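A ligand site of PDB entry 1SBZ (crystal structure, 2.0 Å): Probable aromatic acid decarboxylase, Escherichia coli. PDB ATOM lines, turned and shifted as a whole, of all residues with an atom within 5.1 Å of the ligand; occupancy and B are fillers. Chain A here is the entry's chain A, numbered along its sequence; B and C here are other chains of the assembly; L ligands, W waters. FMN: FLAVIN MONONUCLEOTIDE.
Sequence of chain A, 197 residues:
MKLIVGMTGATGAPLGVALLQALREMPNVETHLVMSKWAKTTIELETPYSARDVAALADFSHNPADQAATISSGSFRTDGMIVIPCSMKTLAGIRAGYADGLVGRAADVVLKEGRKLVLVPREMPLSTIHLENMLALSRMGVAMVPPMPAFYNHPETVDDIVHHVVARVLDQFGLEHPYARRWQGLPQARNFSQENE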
ATOM      1  N   THR A   8       8.109  17.546  11.033  1.00  0.00           N
ATOM      2  CA  THR A   8       6.975  17.351  11.893  1.00  0.00           C
ATOM      3  C   THR A   8       5.733  17.230  11.015  1.00  0.00           C
ATOM      4  O   THR A   8       5.737  17.663   9.859  1.00  0.00           O
ATOM      5  CB  THR A   8       6.944  18.560  12.858  1.00  0.00           C
ATOM      6  OG1 THR A   8       7.568  18.203  14.109  1.00  0.00           O
ATOM      7  CG2 THR A   8       5.599  18.895  13.236  1.00  0.00           C
ATOM      8  N   GLY A   9       4.678  16.641  11.563  1.00  0.00           N
ATOM      9  CA  GLY A   9       3.470  16.291  10.805  1.00  0.00           C
ATOM     10  C   GLY A   9       2.467  17.402  10.536  1.00  0.00           C
ATOM     11  O   GLY A   9       1.265  17.163  10.579  1.00  0.00           O
ATOM     12  N   ALA A  10       2.951  18.604  10.271  1.00  0.00           N
ATOM     13  CA  ALA A  10       2.081  19.660   9.741  1.00  0.00           C
ATOM     14  C   ALA A  10       2.138  19.553   8.222  1.00  0.00           C
ATOM     15  O   ALA A  10       3.148  19.114   7.666  1.00  0.00           O
ATOM     16  CB  ALA A  10       2.555  21.030  10.193  1.00  0.00           C
ATOM     17  N   THR A  11       1.067  19.953   7.541  1.00  0.00           N
ATOM     18  CA  THR A  11       1.121  20.001   6.102  1.00  0.00           C
ATOM     19  C   THR A  11       2.223  20.984   5.674  1.00  0.00           C
ATOM     20  O   THR A  11       2.394  22.051   6.261  1.00  0.00           O
ATOM     21  CB  THR A  11      -0.256  20.293   5.466  1.00  0.00           C
ATOM     22  OG1 THR A  11      -0.097  20.423   4.048  1.00  0.00           O
ATOM     23  CG2 THR A  11      -0.810  21.658   5.884  1.00  0.00           C
ATOM     24  N   SER A  36       9.660  13.123  12.565  1.00  0.00           N
ATOM     25  CA  SER A  36       8.640  12.566  13.448  1.00  0.00           C
ATOM     26  C   SER A  36       7.833  11.495  12.708  1.00  0.00           C
ATOM     27  O   SER A  36       7.778  11.484  11.476  1.00  0.00           O
ATOM     28  CB  SER A  36       7.691  13.666  13.944  1.00  0.00           C
ATOM     29  OG  SER A  36       6.652  13.901  13.011  1.00  0.00           O
ATOM     30  N   TRP A  38       4.601  11.234  12.288  1.00  0.00           N
ATOM     31  CA  TRP A  38       3.593  11.822  11.403  1.00  0.00           C
ATOM     32  C   TRP A  38       4.180  12.612  10.237  1.00  0.00           C
ATOM     33  O   TRP A  38       3.500  12.816   9.232  1.00  0.00           O
ATOM     34  CB  TRP A  38       2.539  12.615  12.202  1.00  0.00           C
ATOM     35  CG  TRP A  38       1.567  11.702  12.884  1.00  0.00           C
ATOM     36  CD1 TRP A  38       1.561  11.341  14.206  1.00  0.00           C
ATOM     37  CD2 TRP A  38       0.480  10.995  12.270  1.00  0.00           C
ATOM     38  NE1 TRP A  38       0.528  10.466  14.451  1.00  0.00           N
ATOM     39  CE2 TRP A  38      -0.149  10.230  13.279  1.00  0.00           C
ATOM     40  CE3 TRP A  38      -0.036  10.939  10.968  1.00  0.00           C
ATOM     41  CZ2 TRP A  38      -1.259   9.423  13.021  1.00  0.00           C
ATOM     42  CZ3 TRP A  38      -1.139  10.128  10.722  1.00  0.00           C
ATOM     43  CH2 TRP A  38      -1.739   9.385  11.737  1.00  0.00           C
ATOM     44  N   ALA A  39       5.434  13.034  10.370  1.00  0.00           N
ATOM     45  CA  ALA A  39       6.145  13.708   9.279  1.00  0.00           C
ATOM     46  C   ALA A  39       6.377  12.743   8.110  1.00  0.00           C
ATOM     47  O   ALA A  39       6.297  13.157   6.957  1.00  0.00           O
ATOM     48  CB  ALA A  39       7.455  14.287   9.760  1.00  0.00           C
ATOM     49  N   THR A  42       3.231  12.629   6.159  1.00  0.00           N
ATOM     50  CA  THR A  42       3.083  13.858   5.418  1.00  0.00           C
ATOM     51  C   THR A  42       4.044  13.934   4.228  1.00  0.00           C
ATOM     52  O   THR A  42       3.675  14.412   3.159  1.00  0.00           O
ATOM     53  CB  THR A  42       3.303  15.048   6.381  1.00  0.00           C
ATOM     54  OG1 THR A  42       2.319  14.974   7.430  1.00  0.00           O
ATOM     55  CG2 THR A  42       2.969  16.348   5.713  1.00  0.00           C
ATOM     56  N   LEU A  45       2.615  11.461   1.559  1.00  0.00           N
ATOM     57  CA  LEU A  45       1.395  12.005   0.960  1.00  0.00           C
ATOM     58  C   LEU A  45       1.629  13.247   0.084  1.00  0.00           C
ATOM     59  O   LEU A  45       0.938  13.439  -0.919  1.00  0.00           O
ATOM     60  CB  LEU A  45       0.370  12.320   2.069  1.00  0.00           C
ATOM     61  CG  LEU A  45      -0.837  13.195   1.729  1.00  0.00           C
ATOM     62  CD1 LEU A  45      -2.016  12.362   1.227  1.00  0.00           C
ATOM     63  CD2 LEU A  45      -1.245  14.036   2.942  1.00  0.00           C
ATOM     64  N   GLU A  46       2.592  14.079   0.461  1.00  0.00           N
ATOM     65  CA  GLU A  46       2.733  15.409  -0.152  1.00  0.00           C
ATOM     66  C   GLU A  46       3.896  15.557  -1.141  1.00  0.00           C
ATOM     67  O   GLU A  46       3.932  16.528  -1.912  1.00  0.00           O
ATOM     68  CB  GLU A  46       2.799  16.503   0.921  1.00  0.00           C
ATOM     69  CG  GLU A  46       1.538  16.612   1.764  1.00  0.00           C
ATOM     70  CD  GLU A  46       1.609  17.654   2.869  1.00  0.00           C
ATOM     71  OE1 GLU A  46       2.678  18.261   3.095  1.00  0.00           O
ATOM     72  OE2 GLU A  46       0.570  17.859   3.523  1.00  0.00           O
ATOM     73  N   SER A  87       4.482  21.480  13.681  1.00  0.00           N
ATOM     74  CA  SER A  87       3.080  21.310  14.066  1.00  0.00           C
ATOM     75  C   SER A  87       2.800  22.037  15.378  1.00  0.00           C
ATOM     76  O   SER A  87       3.726  22.363  16.133  1.00  0.00           O
ATOM     77  CB  SER A  87       2.725  19.839  14.237  1.00  0.00           C
ATOM     78  OG  SER A  87       3.353  19.307  15.393  1.00  0.00           O
ATOM     79  N   MET A  88       1.515  22.261  15.646  1.00  0.00           N
ATOM     80  CA  MET A  88       1.072  22.860  16.897  1.00  0.00           C
ATOM     81  C   MET A  88       1.379  21.973  18.095  1.00  0.00           C
ATOM     82  O   MET A  88       1.751  22.477  19.151  1.00  0.00           O
ATOM     83  CB  MET A  88      -0.413  23.230  16.827  1.00  0.00           C
ATOM     84  CG  MET A  88      -0.726  24.324  15.789  1.00  0.00           C
ATOM     85  SD  MET A  88       0.327  25.959  15.985  1.00  0.00           S
ATOM     86  CE  MET A  88       1.778  25.621  14.649  1.00  0.00           C
ATOM     87  N   LYS A  89       1.246  20.661  17.907  1.00  0.00           N
ATOM     88  CA  LYS A  89       1.595  19.691  18.946  1.00  0.00           C
ATOM     89  C   LYS A  89       3.095  19.754  19.317  1.00  0.00           C
ATOM     90  O   LYS A  89       3.456  19.780  20.498  1.00  0.00           O
ATOM     91  CB  LYS A  89       1.141  18.262  18.549  1.00  0.00           C
ATOM     92  CG  LYS A  89       2.224  17.215  18.388  1.00  0.00           C
ATOM     93  CD  LYS A  89       2.419  16.409  19.642  1.00  0.00           C
ATOM     94  CE  LYS A  89       3.807  15.780  19.677  1.00  0.00           C
ATOM     95  NZ  LYS A  89       3.962  14.536  18.901  1.00  0.00           N
ATOM     96  N   THR A  90       3.979  19.818  18.320  1.00  0.00           N
ATOM     97  CA  THR A  90       5.410  19.922  18.600  1.00  0.00           C
ATOM     98  C   THR A  90       5.752  21.278  19.201  1.00  0.00           C
ATOM     99  O   THR A  90       6.535  21.374  20.136  1.00  0.00           O
ATOM    100  CB  THR A  90       6.252  19.602  17.345  1.00  0.00           C
ATOM    101  OG1 THR A  90       6.286  18.179  17.152  1.00  0.00           O
ATOM    102  CG2 THR A  90       7.722  19.931  17.596  1.00  0.00           C
ATOM    103  N   ARG A 122       3.100  25.965  11.313  1.00  0.00           N
ATOM    104  CA  ARG A 122       2.053  25.937  10.298  1.00  0.00           C
ATOM    105  C   ARG A 122       0.752  25.354  10.839  1.00  0.00           C
ATOM    106  O   ARG A 122       0.673  24.191  11.232  1.00  0.00           O
ATOM    107  CB  ARG A 122       2.533  25.170   9.037  1.00  0.00           C
ATOM    108  CG  ARG A 122       1.671  25.402   7.791  1.00  0.00           C
ATOM    109  CD  ARG A 122       0.431  24.536   7.727  1.00  0.00           C
ATOM    110  NE  ARG A 122      -0.550  24.997   6.739  1.00  0.00           N
ATOM    111  CZ  ARG A 122      -1.857  24.764   6.842  1.00  0.00           C
ATOM    112  NH1 ARG A 122      -2.326  24.097   7.878  1.00  0.00           N
ATOM    113  NH2 ARG A 122      -2.694  25.219   5.907  1.00  0.00           N
ATOM    114  N   GLU A 123      -0.267  26.195  10.838  1.00  0.00           N
ATOM    115  CA  GLU A 123      -1.635  25.855  11.189  1.00  0.00           C
ATOM    116  C   GLU A 123      -2.485  27.062  10.810  1.00  0.00           C
ATOM    117  O   GLU A 123      -1.979  28.190  10.751  1.00  0.00           O
ATOM    118  CB  GLU A 123      -1.775  25.558  12.679  1.00  0.00           C
ATOM    119  CG  GLU A 123      -3.172  25.082  13.115  1.00  0.00           C
ATOM    120  CD  GLU A 123      -3.643  23.832  12.379  1.00  0.00           C
ATOM    121  OE1 GLU A 123      -4.099  23.942  11.217  1.00  0.00           O
ATOM    122  OE2 GLU A 123      -3.603  22.744  12.975  1.00  0.00           O
ATOM    123  N   GLN B  67      -4.445  10.464  13.687  1.00  0.00           N
ATOM    124  CA  GLN B  67      -4.384  11.901  13.388  1.00  0.00           C
ATOM    125  C   GLN B  67      -4.854  12.227  11.958  1.00  0.00           C
ATOM    126  O   GLN B  67      -4.879  13.394  11.553  1.00  0.00           O
ATOM    127  CB  GLN B  67      -2.983  12.480  13.645  1.00  0.00           C
ATOM    128  CG  GLN B  67      -2.407  12.250  15.058  1.00  0.00           C
ATOM    129  CD  GLN B  67      -3.183  12.976  16.154  1.00  0.00           C
ATOM    130  OE1 GLN B  67      -2.604  13.750  16.940  1.00  0.00           O
ATOM    131  NE2 GLN B  67      -4.494  12.744  16.216  1.00  0.00           N
ATOM    132  N   ALA B  68      -5.233  11.196  11.201  1.00  0.00           N
ATOM    133  CA  ALA B  68      -5.683  11.391   9.819  1.00  0.00           C
ATOM    134  C   ALA B  68      -7.188  11.171   9.661  1.00  0.00           C
ATOM    135  O   ALA B  68      -7.709  11.184   8.542  1.00  0.00           O
ATOM    136  CB  ALA B  68      -4.893  10.496   8.858  1.00  0.00           C
ATOM    137  N   SER B  72     -10.034  15.288  12.473  1.00  0.00           N
ATOM    138  CA  SER B  72      -8.731  15.892  12.670  1.00  0.00           C
ATOM    139  C   SER B  72      -8.552  17.091  11.736  1.00  0.00           C
ATOM    140  O   SER B  72      -7.617  17.878  11.881  1.00  0.00           O
ATOM    141  CB  SER B  72      -7.633  14.871  12.438  1.00  0.00           C
ATOM    142  OG  SER B  72      -6.357  15.459  12.525  1.00  0.00           O
ATOM    143  N   ALA B  99      -1.274  18.239  21.218  1.00  0.00           N
ATOM    144  CA  ALA B  99      -2.227  17.396  20.499  1.00  0.00           C
ATOM    145  C   ALA B  99      -1.574  16.097  20.005  1.00  0.00           C
ATOM    146  O   ALA B  99      -1.409  15.894  18.785  1.00  0.00           O
ATOM    147  CB  ALA B  99      -2.834  18.182  19.336  1.00  0.00           C
ATOM    148  N   ASP B 100      -1.213  15.223  20.956  1.00  0.00           N
ATOM    149  CA  ASP B 100      -0.421  14.019  20.691  1.00  0.00           C
ATOM    150  C   ASP B 100      -1.254  12.847  20.126  1.00  0.00           C
ATOM    151  O   ASP B 100      -0.712  11.997  19.417  1.00  0.00           O
ATOM    152  CB  ASP B 100       0.295  13.570  21.967  1.00  0.00           C
ATOM    153  CG  ASP B 100       1.368  12.493  21.706  1.00  0.00           C
ATOM    154  OD1 ASP B 100       2.054  12.547  20.649  1.00  0.00           O
ATOM    155  OD2 ASP B 100       1.594  11.573  22.518  1.00  0.00           O
ATOM    156  N   ARG B 105      -6.036  16.340  19.406  1.00  0.00           N
ATOM    157  CA  ARG B 105      -6.061  16.972  18.090  1.00  0.00           C
ATOM    158  C   ARG B 105      -7.467  17.465  17.707  1.00  0.00           C
ATOM    159  O   ARG B 105      -7.618  18.609  17.297  1.00  0.00           O
ATOM    160  CB  ARG B 105      -5.505  16.036  17.003  1.00  0.00           C
ATOM    161  CG  ARG B 105      -5.659  16.551  15.565  1.00  0.00           C
ATOM    162  CD  ARG B 105      -4.891  17.840  15.244  1.00  0.00           C
ATOM    163  NE  ARG B 105      -5.128  18.268  13.856  1.00  0.00           N
ATOM    164  CZ  ARG B 105      -4.739  19.427  13.350  1.00  0.00           C
ATOM    165  NH1 ARG B 105      -4.102  20.321  14.096  1.00  0.00           N
ATOM    166  NH2 ARG B 105      -5.006  19.713  12.082  1.00  0.00           N
ATOM    167  N   TYR C 152      -1.564  19.195   1.358  1.00  0.00           N
ATOM    168  CA  TYR C 152      -2.222  17.872   1.379  1.00  0.00           C
ATOM    169  C   TYR C 152      -3.163  17.654   0.190  1.00  0.00           C
ATOM    170  O   TYR C 152      -3.400  16.516  -0.213  1.00  0.00           O
ATOM    171  CB  TYR C 152      -2.945  17.618   2.715  1.00  0.00           C
ATOM    172  CG  TYR C 152      -3.953  18.677   3.112  1.00  0.00           C
ATOM    173  CD1 TYR C 152      -3.624  19.666   4.034  1.00  0.00           C
ATOM    174  CD2 TYR C 152      -5.240  18.688   2.561  1.00  0.00           C
ATOM    175  CE1 TYR C 152      -4.545  20.645   4.392  1.00  0.00           C
ATOM    176  CE2 TYR C 152      -6.161  19.668   2.919  1.00  0.00           C
ATOM    177  CZ  TYR C 152      -5.813  20.647   3.835  1.00  0.00           C
ATOM    178  OH  TYR C 152      -6.727  21.604   4.189  1.00  0.00           O
HETATM  179  N1  FMN L   1      -1.067  19.723  12.637  1.00  0.00           N
HETATM  180  C2  FMN L   1      -0.770  21.065  12.669  1.00  0.00           C
HETATM  181  O2  FMN L   1      -0.495  21.588  13.741  1.00  0.00           O
HETATM  182  N3  FMN L   1      -0.762  21.811  11.493  1.00  0.00           N
HETATM  183  C4  FMN L   1      -1.072  21.202  10.293  1.00  0.00           C
HETATM  184  O4  FMN L   1      -1.186  21.880   9.268  1.00  0.00           O
HETATM  185  C4A FMN L   1      -1.378  19.838  10.268  1.00  0.00           C
HETATM  186  N5  FMN L   1      -1.686  19.221   9.072  1.00  0.00           N
HETATM  187  C5A FMN L   1      -1.986  17.865   9.038  1.00  0.00           C
HETATM  188  C6  FMN L   1      -2.291  17.276   7.806  1.00  0.00           C
HETATM  189  C7  FMN L   1      -2.592  15.916   7.718  1.00  0.00           C
HETATM  190  C7M FMN L   1      -2.176  15.248   6.436  1.00  0.00           C
HETATM  191  C8  FMN L   1      -2.611  15.157   8.897  1.00  0.00           C
HETATM  192  C8M FMN L   1      -2.688  13.660   8.838  1.00  0.00           C
HETATM  193  C9  FMN L   1      -2.306  15.746  10.129  1.00  0.00           C
HETATM  194  C9A FMN L   1      -1.991  17.114  10.202  1.00  0.00           C
HETATM  195  N10 FMN L   1      -1.698  17.724  11.413  1.00  0.00           N
HETATM  196  C10 FMN L   1      -1.384  19.084  11.449  1.00  0.00           C
HETATM  197  C1' FMN L   1      -1.915  16.969  12.694  1.00  0.00           C
HETATM  198  C2' FMN L   1      -0.570  16.493  13.253  1.00  0.00           C
HETATM  199  O2' FMN L   1       0.060  15.651  12.317  1.00  0.00           O
HETATM  200  C3' FMN L   1      -0.740  15.781  14.598  1.00  0.00           C
HETATM  201  O3' FMN L   1      -1.063  16.743  15.579  1.00  0.00           O
HETATM  202  C4' FMN L   1       0.497  14.990  15.042  1.00  0.00           C
HETATM  203  O4' FMN L   1       0.270  14.484  16.343  1.00  0.00           O
HETATM  204  C5' FMN L   1       1.754  15.838  15.063  1.00  0.00           C
HETATM  205  O5' FMN L   1       2.801  15.107  15.649  1.00  0.00           O
HETATM  206  P   FMN L   1       4.328  15.507  15.382  1.00  0.00           P
HETATM  207  O1P FMN L   1       5.198  14.680  16.294  1.00  0.00           O
HETATM  208  O2P FMN L   1       4.551  16.978  15.680  1.00  0.00           O
HETATM  209  O3P FMN L   1       4.633  15.242  13.931  1.00  0.00           O
HETATM  210  O   HOH W   1       1.531  12.576  17.671  1.00  0.00           O
HETATM  211  O   HOH W   2      -4.506  21.719  10.053  1.00  0.00           O
HETATM  212  O   HOH W   3       7.488  15.678  17.056  1.00  0.00           O
HETATM  213  O   HOH W   4      -0.650  19.629  15.809  1.00  0.00           O
HETATM  214  O   HOH W   5       4.803  11.968  15.361  1.00  0.00           O
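Water W3 lies within hydrogen-bond range of O1P of the ligand and OG1 of Thr 90. Water W1 lies within hydrogen-bond range of O4' of the ligand (2.6 Å), O of Asp 100 of chain B (2.9 Å) and NZ of Lys 89 (3.4 Å). Water W4 lies within hydrogen-bond range of O2 of the ligand (2.9 Å), N of Lys 89 (3.0 Å) and N of Met 88 (3.4 Å). Water W5 bridges O1P of the ligand (2.9 Å) and N of Trp 38 (3.2 Å). Water W2 lies within hydrogen-bond range of the side-chain carboxylate (OE1) of Glu 123 (2.5 Å), the guanidinium group (NH2) of Arg 105 of chain B (2.9 Å) and an oxygen (O4) of the ligand (3.4 Å).
Thr 8 touches the ligand. CA of Ala 10 touches C4A of the ligand, 3.5 Å away. CB of Trp 38 touches O3P of the ligand, 3.8 Å away. Leu 45 touches the ligand. CB of Ala 68 of chain B touches C8M of the ligand (3.9 Å).
OE2 of Glu 123 sits close to N3 of the ligand, 3.3 Å away. The side-chain hydroxyl (OG) of Ser 87 sits at hydrogen-bond distance from an oxygen (O2P) of the ligand (2.6 Å). An oxygen (O2) of the ligand sits at hydrogen-bond distance from the backbone NH of Met 88, 2.8 Å away. O of Arg 122 sits at hydrogen-bond distance from N3 of the ligand (2.8 Å). O2P of the ligand lies within hydrogen-bond range of OG1 of Thr 90, at 2.6 Å. A nitrogen (N1) of the ligand sits at hydrogen-bond distance from the guanidinium group (NH1) of Arg 105 of chain B, 3.4 Å away. The backbone carbonyl oxygen (O) of Ala 99 of chain B lies within hydrogen-bond range of an oxygen (O4') of the ligand, 3.3 Å away. The backbone NH of Gly 9 lies within hydrogen-bond range of an oxygen (O3P) of the ligand (2.8 Å). The side-chain amide oxygen (OE1) of Gln 67 of chain B lies within hydrogen-bond range of an oxygen (O4') of the ligand, 3.0 Å away. N5 of the ligand is in hydrogen-bond range of N of Thr 11 (3.2 Å). An oxygen (O4) of the ligand is in hydrogen-bond range of the guanidinium group of Arg 122, at 2.9 Å. The side-chain amino group of Lys 89 lies within salt-bridge range of an oxygen (O1P) of the ligand. The backbone carbonyl oxygen (O) of Gly 9 lies within hydrogen-bond range of an oxygen (O2') of the ligand (2.6 Å). The side-chain hydroxyl (OG) of Ser 36 sits at hydrogen-bond distance from an oxygen (O3P) of the ligand, 2.6 Å away.
The side-chain hydroxyl (OG) of Ser 36 sits close to the backbone NH (N) of Trp 38, 3.4 Å away. The side-chain hydroxyl (OG1) of Thr 11 sits at hydrogen-bond distance from the side-chain carboxylate (OE2) of Glu 46 (2.7 Å). OE1 of Gln 67 of chain B sits close to O of Ala 99 of chain B (3.1 Å). OG1 of Thr 90 sits at hydrogen-bond distance from OG1 of Thr 8, 3.3 Å away. The backbone carbonyl oxygen of Ser 72 of chain B is in hydrogen-bond range of the guanidinium group of Arg 105 of chain B (3.2 Å). The side-chain carboxylate (OD1) of Asp 100 of chain B lies within salt-bridge range of the side-chain amino group (NZ) of Lys 89 (3.3 Å). The guanidinium group (NH1) of Arg 105 of chain B is in salt-bridge range of the side-chain carboxylate (OE2) of Glu 123. The side-chain hydroxyl of Ser 36 sits at hydrogen-bond distance from the backbone NH of Ala 39 (3.0 Å).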
